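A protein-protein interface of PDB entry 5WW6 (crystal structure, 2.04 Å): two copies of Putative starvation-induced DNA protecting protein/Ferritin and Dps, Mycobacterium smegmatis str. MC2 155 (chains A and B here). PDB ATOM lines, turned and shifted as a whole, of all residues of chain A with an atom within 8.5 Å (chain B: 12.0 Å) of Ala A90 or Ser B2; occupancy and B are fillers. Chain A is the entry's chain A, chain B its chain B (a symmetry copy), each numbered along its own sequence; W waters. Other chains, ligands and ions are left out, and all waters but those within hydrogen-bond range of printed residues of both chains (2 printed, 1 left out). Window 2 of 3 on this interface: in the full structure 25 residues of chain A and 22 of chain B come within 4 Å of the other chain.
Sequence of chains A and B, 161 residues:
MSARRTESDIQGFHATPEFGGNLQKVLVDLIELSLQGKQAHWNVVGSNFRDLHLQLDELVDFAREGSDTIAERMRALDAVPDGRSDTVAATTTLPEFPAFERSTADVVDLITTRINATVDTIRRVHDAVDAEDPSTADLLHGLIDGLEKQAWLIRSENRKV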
ATOM      1  N   VAL A  28     -21.787 -11.394  18.092  1.00  0.00           N
ATOM      2  CA  VAL A  28     -20.412 -10.867  17.999  1.00  0.00           C
ATOM      3  C   VAL A  28     -19.362 -11.893  18.413  1.00  0.00           C
ATOM      4  O   VAL A  28     -18.303 -11.966  17.805  1.00  0.00           O
ATOM      5  CB  VAL A  28     -20.188  -9.512  18.723  1.00  0.00           C
ATOM      6  CG1 VAL A  28     -21.033  -8.421  18.070  1.00  0.00           C
ATOM      7  CG2 VAL A  28     -20.464  -9.596  20.228  1.00  0.00           C
ATOM      8  N   ASP A  29     -19.683 -12.709  19.413  1.00  0.00           N
ATOM      9  CA  ASP A  29     -18.763 -13.729  19.882  1.00  0.00           C
ATOM     10  C   ASP A  29     -18.618 -14.875  18.895  1.00  0.00           C
ATOM     11  O   ASP A  29     -17.528 -15.402  18.741  1.00  0.00           O
ATOM     12  CB  ASP A  29     -19.127 -14.202  21.294  1.00  0.00           C
ATOM     13  CG  ASP A  29     -18.708 -13.193  22.362  1.00  0.00           C
ATOM     14  OD1 ASP A  29     -17.987 -12.220  22.039  1.00  0.00           O
ATOM     15  OD2 ASP A  29     -19.078 -13.379  23.526  1.00  0.00           O
ATOM     16  N   GLU A  32     -16.488 -13.337  16.049  1.00  0.00           N
ATOM     17  CA  GLU A  32     -15.113 -13.282  16.551  1.00  0.00           C
ATOM     18  C   GLU A  32     -14.477 -14.671  16.570  1.00  0.00           C
ATOM     19  O   GLU A  32     -13.329 -14.832  16.146  1.00  0.00           O
ATOM     20  CB  GLU A  32     -15.034 -12.624  17.934  1.00  0.00           C
ATOM     21  CG  GLU A  32     -13.629 -12.589  18.558  1.00  0.00           C
ATOM     22  CD  GLU A  32     -12.637 -11.660  17.850  1.00  0.00           C
ATOM     23  OE1 GLU A  32     -12.998 -10.987  16.866  1.00  0.00           O
ATOM     24  OE2 GLU A  32     -11.467 -11.610  18.278  1.00  0.00           O
ATOM     25  N   ARG A  84     -20.501  -5.935  11.950  1.00  0.00           N
ATOM     26  CA  ARG A  84     -19.403  -5.181  11.337  1.00  0.00           C
ATOM     27  C   ARG A  84     -18.120  -5.346  12.147  1.00  0.00           C
ATOM     28  O   ARG A  84     -18.178  -5.542  13.367  1.00  0.00           O
ATOM     29  CB  ARG A  84     -19.775  -3.695  11.174  1.00  0.00           C
ATOM     30  CG  ARG A  84     -21.000  -3.458  10.291  1.00  0.00           C
ATOM     31  CD  ARG A  84     -21.501  -2.019  10.344  1.00  0.00           C
ATOM     32  NE  ARG A  84     -21.878  -1.600  11.701  1.00  0.00           N
ATOM     33  CZ  ARG A  84     -21.955  -0.335  12.119  1.00  0.00           C
ATOM     34  NH1 ARG A  84     -21.685   0.679  11.298  1.00  0.00           N
ATOM     35  NH2 ARG A  84     -22.283  -0.086  13.382  1.00  0.00           N
ATOM     36  N   SER A  85     -16.973  -5.274  11.471  1.00  0.00           N
ATOM     37  CA  SER A  85     -15.671  -5.532  12.105  1.00  0.00           C
ATOM     38  C   SER A  85     -15.408  -4.668  13.343  1.00  0.00           C
ATOM     39  O   SER A  85     -14.932  -5.179  14.365  1.00  0.00           O
ATOM     40  CB  SER A  85     -14.520  -5.400  11.110  1.00  0.00           C
ATOM     41  OG  SER A  85     -14.542  -4.146  10.456  1.00  0.00           O
ATOM     42  N   ASP A  86     -15.738  -3.378  13.250  1.00  0.00           N
ATOM     43  CA  ASP A  86     -15.518  -2.438  14.361  1.00  0.00           C
ATOM     44  C   ASP A  86     -16.322  -2.821  15.594  1.00  0.00           C
ATOM     45  O   ASP A  86     -15.802  -2.780  16.706  1.00  0.00           O
ATOM     46  CB  ASP A  86     -15.846  -0.997  13.946  1.00  0.00           C
ATOM     47  CG  ASP A  86     -14.889  -0.474  12.908  1.00  0.00           C
ATOM     48  OD1 ASP A  86     -13.851   0.085  13.291  1.00  0.00           O
ATOM     49  OD2 ASP A  86     -15.170  -0.626  11.701  1.00  0.00           O
ATOM     50  N   THR A  87     -17.580  -3.196  15.378  1.00  0.00           N
ATOM     51  CA  THR A  87     -18.480  -3.593  16.458  1.00  0.00           C
ATOM     52  C   THR A  87     -18.000  -4.888  17.101  1.00  0.00           C
ATOM     53  O   THR A  87     -17.900  -4.962  18.331  1.00  0.00           O
ATOM     54  CB  THR A  87     -19.928  -3.736  15.946  1.00  0.00           C
ATOM     55  OG1 THR A  87     -20.347  -2.482  15.399  1.00  0.00           O
ATOM     56  CG2 THR A  87     -20.899  -4.164  17.084  1.00  0.00           C
ATOM     57  N   VAL A  88     -17.693  -5.886  16.266  1.00  0.00           N
ATOM     58  CA  VAL A  88     -17.161  -7.174  16.731  1.00  0.00           C
ATOM     59  C   VAL A  88     -15.918  -6.958  17.606  1.00  0.00           C
ATOM     60  O   VAL A  88     -15.898  -7.414  18.748  1.00  0.00           O
ATOM     61  CB  VAL A  88     -16.902  -8.167  15.563  1.00  0.00           C
ATOM     62  CG1 VAL A  88     -16.181  -9.420  16.045  1.00  0.00           C
ATOM     63  CG2 VAL A  88     -18.213  -8.564  14.884  1.00  0.00           C
ATOM     64  N   ALA A  89     -14.926  -6.228  17.095  1.00  0.00           N
ATOM     65  CA  ALA A  89     -13.696  -5.919  17.849  1.00  0.00           C
ATOM     66  C   ALA A  89     -13.967  -5.171  19.157  1.00  0.00           C
ATOM     67  O   ALA A  89     -13.390  -5.515  20.183  1.00  0.00           O
ATOM     68  CB  ALA A  89     -12.698  -5.144  16.992  1.00  0.00           C
ATOM     69  N   ALA A  90     -14.861  -4.184  19.108  1.00  0.00           N
ATOM     70  CA  ALA A  90     -15.181  -3.335  20.264  1.00  0.00           C
ATOM     71  C   ALA A  90     -16.008  -4.015  21.356  1.00  0.00           C
ATOM     72  O   ALA A  90     -15.963  -3.581  22.510  1.00  0.00           O
ATOM     73  CB  ALA A  90     -15.879  -2.059  19.813  1.00  0.00           C
ATOM     74  N   THR A  91     -16.757  -5.061  20.998  1.00  0.00           N
ATOM     75  CA  THR A  91     -17.750  -5.641  21.915  1.00  0.00           C
ATOM     76  C   THR A  91     -17.632  -7.143  22.201  1.00  0.00           C
ATOM     77  O   THR A  91     -18.298  -7.634  23.118  1.00  0.00           O
ATOM     78  CB  THR A  91     -19.213  -5.323  21.496  1.00  0.00           C
ATOM     79  OG1 THR A  91     -19.537  -6.018  20.280  1.00  0.00           O
ATOM     80  CG2 THR A  91     -19.455  -3.787  21.342  1.00  0.00           C
ATOM     81  N   THR A  92     -16.805  -7.869  21.439  1.00  0.00           N
ATOM     82  CA  THR A  92     -16.561  -9.296  21.735  1.00  0.00           C
ATOM     83  C   THR A  92     -15.990  -9.490  23.144  1.00  0.00           C
ATOM     84  O   THR A  92     -15.228  -8.648  23.632  1.00  0.00           O
ATOM     85  CB  THR A  92     -15.667 -10.009  20.680  1.00  0.00           C
ATOM     86  OG1 THR A  92     -15.623 -11.412  20.967  1.00  0.00           O
ATOM     87  CG2 THR A  92     -14.228  -9.448  20.645  1.00  0.00           C
ATOM     88  N   THR A  93     -16.388 -10.583  23.793  1.00  0.00           N
ATOM     89  CA  THR A  93     -15.874 -10.921  25.127  1.00  0.00           C
ATOM     90  C   THR A  93     -14.698 -11.896  25.046  1.00  0.00           C
ATOM     91  O   THR A  93     -14.053 -12.169  26.056  1.00  0.00           O
ATOM     92  CB  THR A  93     -16.966 -11.507  26.059  1.00  0.00           C
ATOM     93  OG1 THR A  93     -17.351 -12.805  25.596  1.00  0.00           O
ATOM     94  CG2 THR A  93     -18.202 -10.590  26.125  1.00  0.00           C
ATOM     95  N   LEU A  94     -14.421 -12.415  23.848  1.00  0.00           N
ATOM     96  CA  LEU A  94     -13.306 -13.347  23.655  1.00  0.00           C
ATOM     97  C   LEU A  94     -11.958 -12.655  23.873  1.00  0.00           C
ATOM     98  O   LEU A  94     -11.773 -11.531  23.393  1.00  0.00           O
ATOM     99  CB  LEU A  94     -13.342 -13.982  22.250  1.00  0.00           C
ATOM    100  CG  LEU A  94     -14.148 -15.278  22.051  1.00  0.00           C
ATOM    101  CD1 LEU A  94     -15.614 -15.091  22.424  1.00  0.00           C
ATOM    102  CD2 LEU A  94     -14.010 -15.778  20.612  1.00  0.00           C
ATOM    103  N   GLU A  96      -8.315 -11.719  22.880  1.00  0.00           N
ATOM    104  CA  GLU A  96      -7.694 -11.558  21.566  1.00  0.00           C
ATOM    105  C   GLU A  96      -6.867 -12.801  21.223  1.00  0.00           C
ATOM    106  O   GLU A  96      -6.204 -13.367  22.092  1.00  0.00           O
ATOM    107  CB  GLU A  96      -6.816 -10.299  21.580  1.00  0.00           C
ATOM    108  CG  GLU A  96      -6.092  -9.981  20.280  1.00  0.00           C
ATOM    109  CD  GLU A  96      -5.487  -8.587  20.259  1.00  0.00           C
ATOM    110  OE1 GLU A  96      -5.356  -7.965  21.326  1.00  0.00           O
ATOM    111  OE2 GLU A  96      -5.145  -8.104  19.162  1.00  0.00           O
ATOM    112  N   SER B   2     -11.768  -4.354  24.677  1.00  0.00           N
ATOM    113  CA  SER B   2     -12.540  -3.425  25.564  1.00  0.00           C
ATOM    114  C   SER B   2     -13.657  -4.154  26.315  1.00  0.00           C
ATOM    115  O   SER B   2     -13.770  -3.996  27.528  1.00  0.00           O
ATOM    116  CB  SER B   2     -13.048  -2.187  24.809  1.00  0.00           C
ATOM    117  OG  SER B   2     -13.592  -2.523  23.547  1.00  0.00           O
ATOM    118  N   ALA B   3     -14.459  -4.961  25.616  1.00  0.00           N
ATOM    119  CA  ALA B   3     -15.284  -5.967  26.308  1.00  0.00           C
ATOM    120  C   ALA B   3     -14.572  -7.333  26.428  1.00  0.00           C
ATOM    121  O   ALA B   3     -15.126  -8.270  27.007  1.00  0.00           O
ATOM    122  CB  ALA B   3     -16.661  -6.108  25.662  1.00  0.00           C
ATOM    123  N   ARG B   4     -13.344  -7.425  25.903  1.00  0.00           N
ATOM    124  CA  ARG B   4     -12.546  -8.661  25.927  1.00  0.00           C
ATOM    125  C   ARG B   4     -12.212  -9.105  27.350  1.00  0.00           C
ATOM    126  O   ARG B   4     -11.751  -8.305  28.172  1.00  0.00           O
ATOM    127  CB  ARG B   4     -11.251  -8.521  25.112  1.00  0.00           C
ATOM    128  CG  ARG B   4     -11.462  -8.310  23.620  1.00  0.00           C
ATOM    129  CD  ARG B   4     -10.189  -8.543  22.818  1.00  0.00           C
ATOM    130  NE  ARG B   4     -10.396  -8.298  21.387  1.00  0.00           N
ATOM    131  CZ  ARG B   4     -10.747  -9.220  20.485  1.00  0.00           C
ATOM    132  NH1 ARG B   4     -10.903  -8.864  19.214  1.00  0.00           N
ATOM    133  NH2 ARG B   4     -10.944 -10.494  20.830  1.00  0.00           N
ATOM    134  N   ARG B   5     -12.478 -10.378  27.628  1.00  0.00           N
ATOM    135  CA  ARG B   5     -12.072 -11.009  28.882  1.00  0.00           C
ATOM    136  C   ARG B   5     -10.563 -11.239  28.866  1.00  0.00           C
ATOM    137  O   ARG B   5      -9.977 -11.479  27.809  1.00  0.00           O
ATOM    138  CB  ARG B   5     -12.834 -12.314  29.096  1.00  0.00           C
ATOM    139  CG  ARG B   5     -14.311 -12.084  29.379  1.00  0.00           C
ATOM    140  CD  ARG B   5     -15.119 -13.366  29.287  1.00  0.00           C
ATOM    141  NE  ARG B   5     -14.895 -14.233  30.441  1.00  0.00           N
ATOM    142  CZ  ARG B   5     -15.513 -15.393  30.660  1.00  0.00           C
ATOM    143  NH1 ARG B   5     -16.420 -15.862  29.804  1.00  0.00           N
ATOM    144  NH2 ARG B   5     -15.224 -16.083  31.752  1.00  0.00           N
ATOM    145  N   THR B   6      -9.935 -11.141  30.034  1.00  0.00           N
ATOM    146  CA  THR B   6      -8.464 -11.062  30.098  1.00  0.00           C
ATOM    147  C   THR B   6      -7.774 -12.280  30.719  1.00  0.00           C
ATOM    148  O   THR B   6      -6.540 -12.338  30.780  1.00  0.00           O
ATOM    149  CB  THR B   6      -7.976  -9.758  30.777  1.00  0.00           C
ATOM    150  OG1 THR B   6      -8.645  -9.582  32.033  1.00  0.00           O
ATOM    151  CG2 THR B   6      -8.227  -8.542  29.876  1.00  0.00           C
ATOM    152  N   GLU B   7      -8.569 -13.247  31.170  1.00  0.00           N
ATOM    153  CA  GLU B   7      -8.026 -14.513  31.671  1.00  0.00           C
ATOM    154  C   GLU B   7      -7.548 -15.373  30.506  1.00  0.00           C
ATOM    155  O   GLU B   7      -8.182 -15.408  29.446  1.00  0.00           O
ATOM    156  CB  GLU B   7      -9.043 -15.251  32.548  1.00  0.00           C
ATOM    157  CG  GLU B   7     -10.452 -15.264  31.985  1.00  0.00           C
ATOM    158  CD  GLU B   7     -11.518 -15.091  33.042  1.00  0.00           C
ATOM    159  OE1 GLU B   7     -11.549 -15.892  34.001  1.00  0.00           O
ATOM    160  OE2 GLU B   7     -12.334 -14.157  32.901  1.00  0.00           O
HETATM  161  O   HOH W   1     -10.690  -5.584  20.709  1.00  0.00           O
HETATM  162  O   HOH W   2     -17.483 -14.863  27.310  1.00  0.00           O
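Water W2 bridges the side-chain hydroxyl (OG1) of Thr A93 (2.7 Å) and the guanidinium group (NH1) of Arg B5 (2.9 Å).
Water W1 lies within hydrogen-bond range of the backbone carbonyl oxygen of Ala A89 and the guanidinium group of Arg B4.
Among the printed residues, pairs that only touch across the chains: Ala A90 with Ala B3 (3.7 Å), Thr A91 with Ala B3 (3.4 Å), Thr A93 with Ala B3 (3.3 Å), Thr A93 with Arg B4 (3.8 Å) and Glu A96 with Arg B4 (3.5 Å).
OE2 of Glu A32 lies within salt-bridge range of NH2 of Arg B4 (2.8 Å).
The side-chain hydroxyl of Ser B2 is in hydrogen-bond range of the backbone carbonyl oxygen of Ala A90 (2.8 Å).
The backbone NH (N) of Arg B4 is in hydrogen-bond range of the backbone carbonyl oxygen (O) of Thr A92 (3.2 Å).
The backbone NH (N) of Arg B5 sits at hydrogen-bond distance from the backbone carbonyl oxygen (O) of Thr A93, at 2.9 Å.
The guanidinium group of Arg B4 is in hydrogen-bond range of the backbone carbonyl oxygen of Leu A94 (2.9 Å).
The backbone carbonyl oxygen (O) of Thr A92 lies close to the backbone carbonyl oxygen (O) of Ala B3, 3.4 Å away.
Val A28 touches none of the printed residues of chain B.
Printed residues of chain B within 4 Å of Glu A32: Arg B4.
Asp A86 touches none of the printed residues of chain B.
No residue of chain B comes within 4 Å of Thr A87.
No residue of chain B comes within 4 Å of Val A88.
No residue of chain B comes within 4 Å of Ala A89.
Of chain B, only Ser B2 (2.8 Å) and Ala B3 (3.7 Å) come within 4 Å of Ala A90.
Thr A91 touches one residue of chain B.
Printed residues of chain B within 4 Å of Thr A92: Ala B3 and Arg B4.
Printed residues of chain B within 4 Å of Thr A93: Ala B3 (3.3 Å), Arg B4 (3.8 Å) and Arg B5 (2.9 Å).
Printed residues of chain B within 4 Å of Glu A96: Arg B4 (3.5 Å).
Of chain A, only Ala A90, Thr A91, Thr A92 and Thr A93 come within 4 Å of Ala B3.
Printed residues of chain A within 4 Å of Arg B4: Glu A32 (2.8 Å), Thr A92 (3.2 Å), Thr A93 (3.8 Å), Leu A94 (2.9 Å) and Glu A96 (3.5 Å).
Of the printed residues of chain A, Arg B5 touches Thr A93.
No position is printed for both chains.
Of the 11 pairs that touch across the chains among the printed residues, none has its exchanged pair printed and touching as well.
The side-chain carboxylate of Asp A29 is in hydrogen-bond range of the side-chain hydroxyl of Thr A92, 2.7 Å away.
The side-chain carboxylate (OD2) of Asp A29 lies within hydrogen-bond range of the side-chain hydroxyl (OG1) of Thr A93, at 2.8 Å.
The backbone carbonyl oxygen of Thr A87 is in hydrogen-bond range of the side-chain hydroxyl of Thr A91 (2.8 Å).
The side-chain hydroxyl of Thr A92 sits at hydrogen-bond distance from the backbone NH of Leu A94 (3.3 Å).
The guanidinium group of Arg B5 lies within salt-bridge range of the side-chain carboxylate of Glu B7, at 3.6 Å.
Of the 6 printed residues of chain B, 4 touch a printed residue of chain A.
Printed residues of chain B that touch a printed residue of chain A: Ser B2, Ala B3, Arg B4 and Arg B5.
Hydrophobic or aromatic side chains of chain B within 4 Å of the printed part of chain A: Ala B3.
Among the printed residues, Asp or Glu carboxylates within 4 Å of a Lys or Arg side-chain nitrogen of the other chain: Glu A32 with Arg B4.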
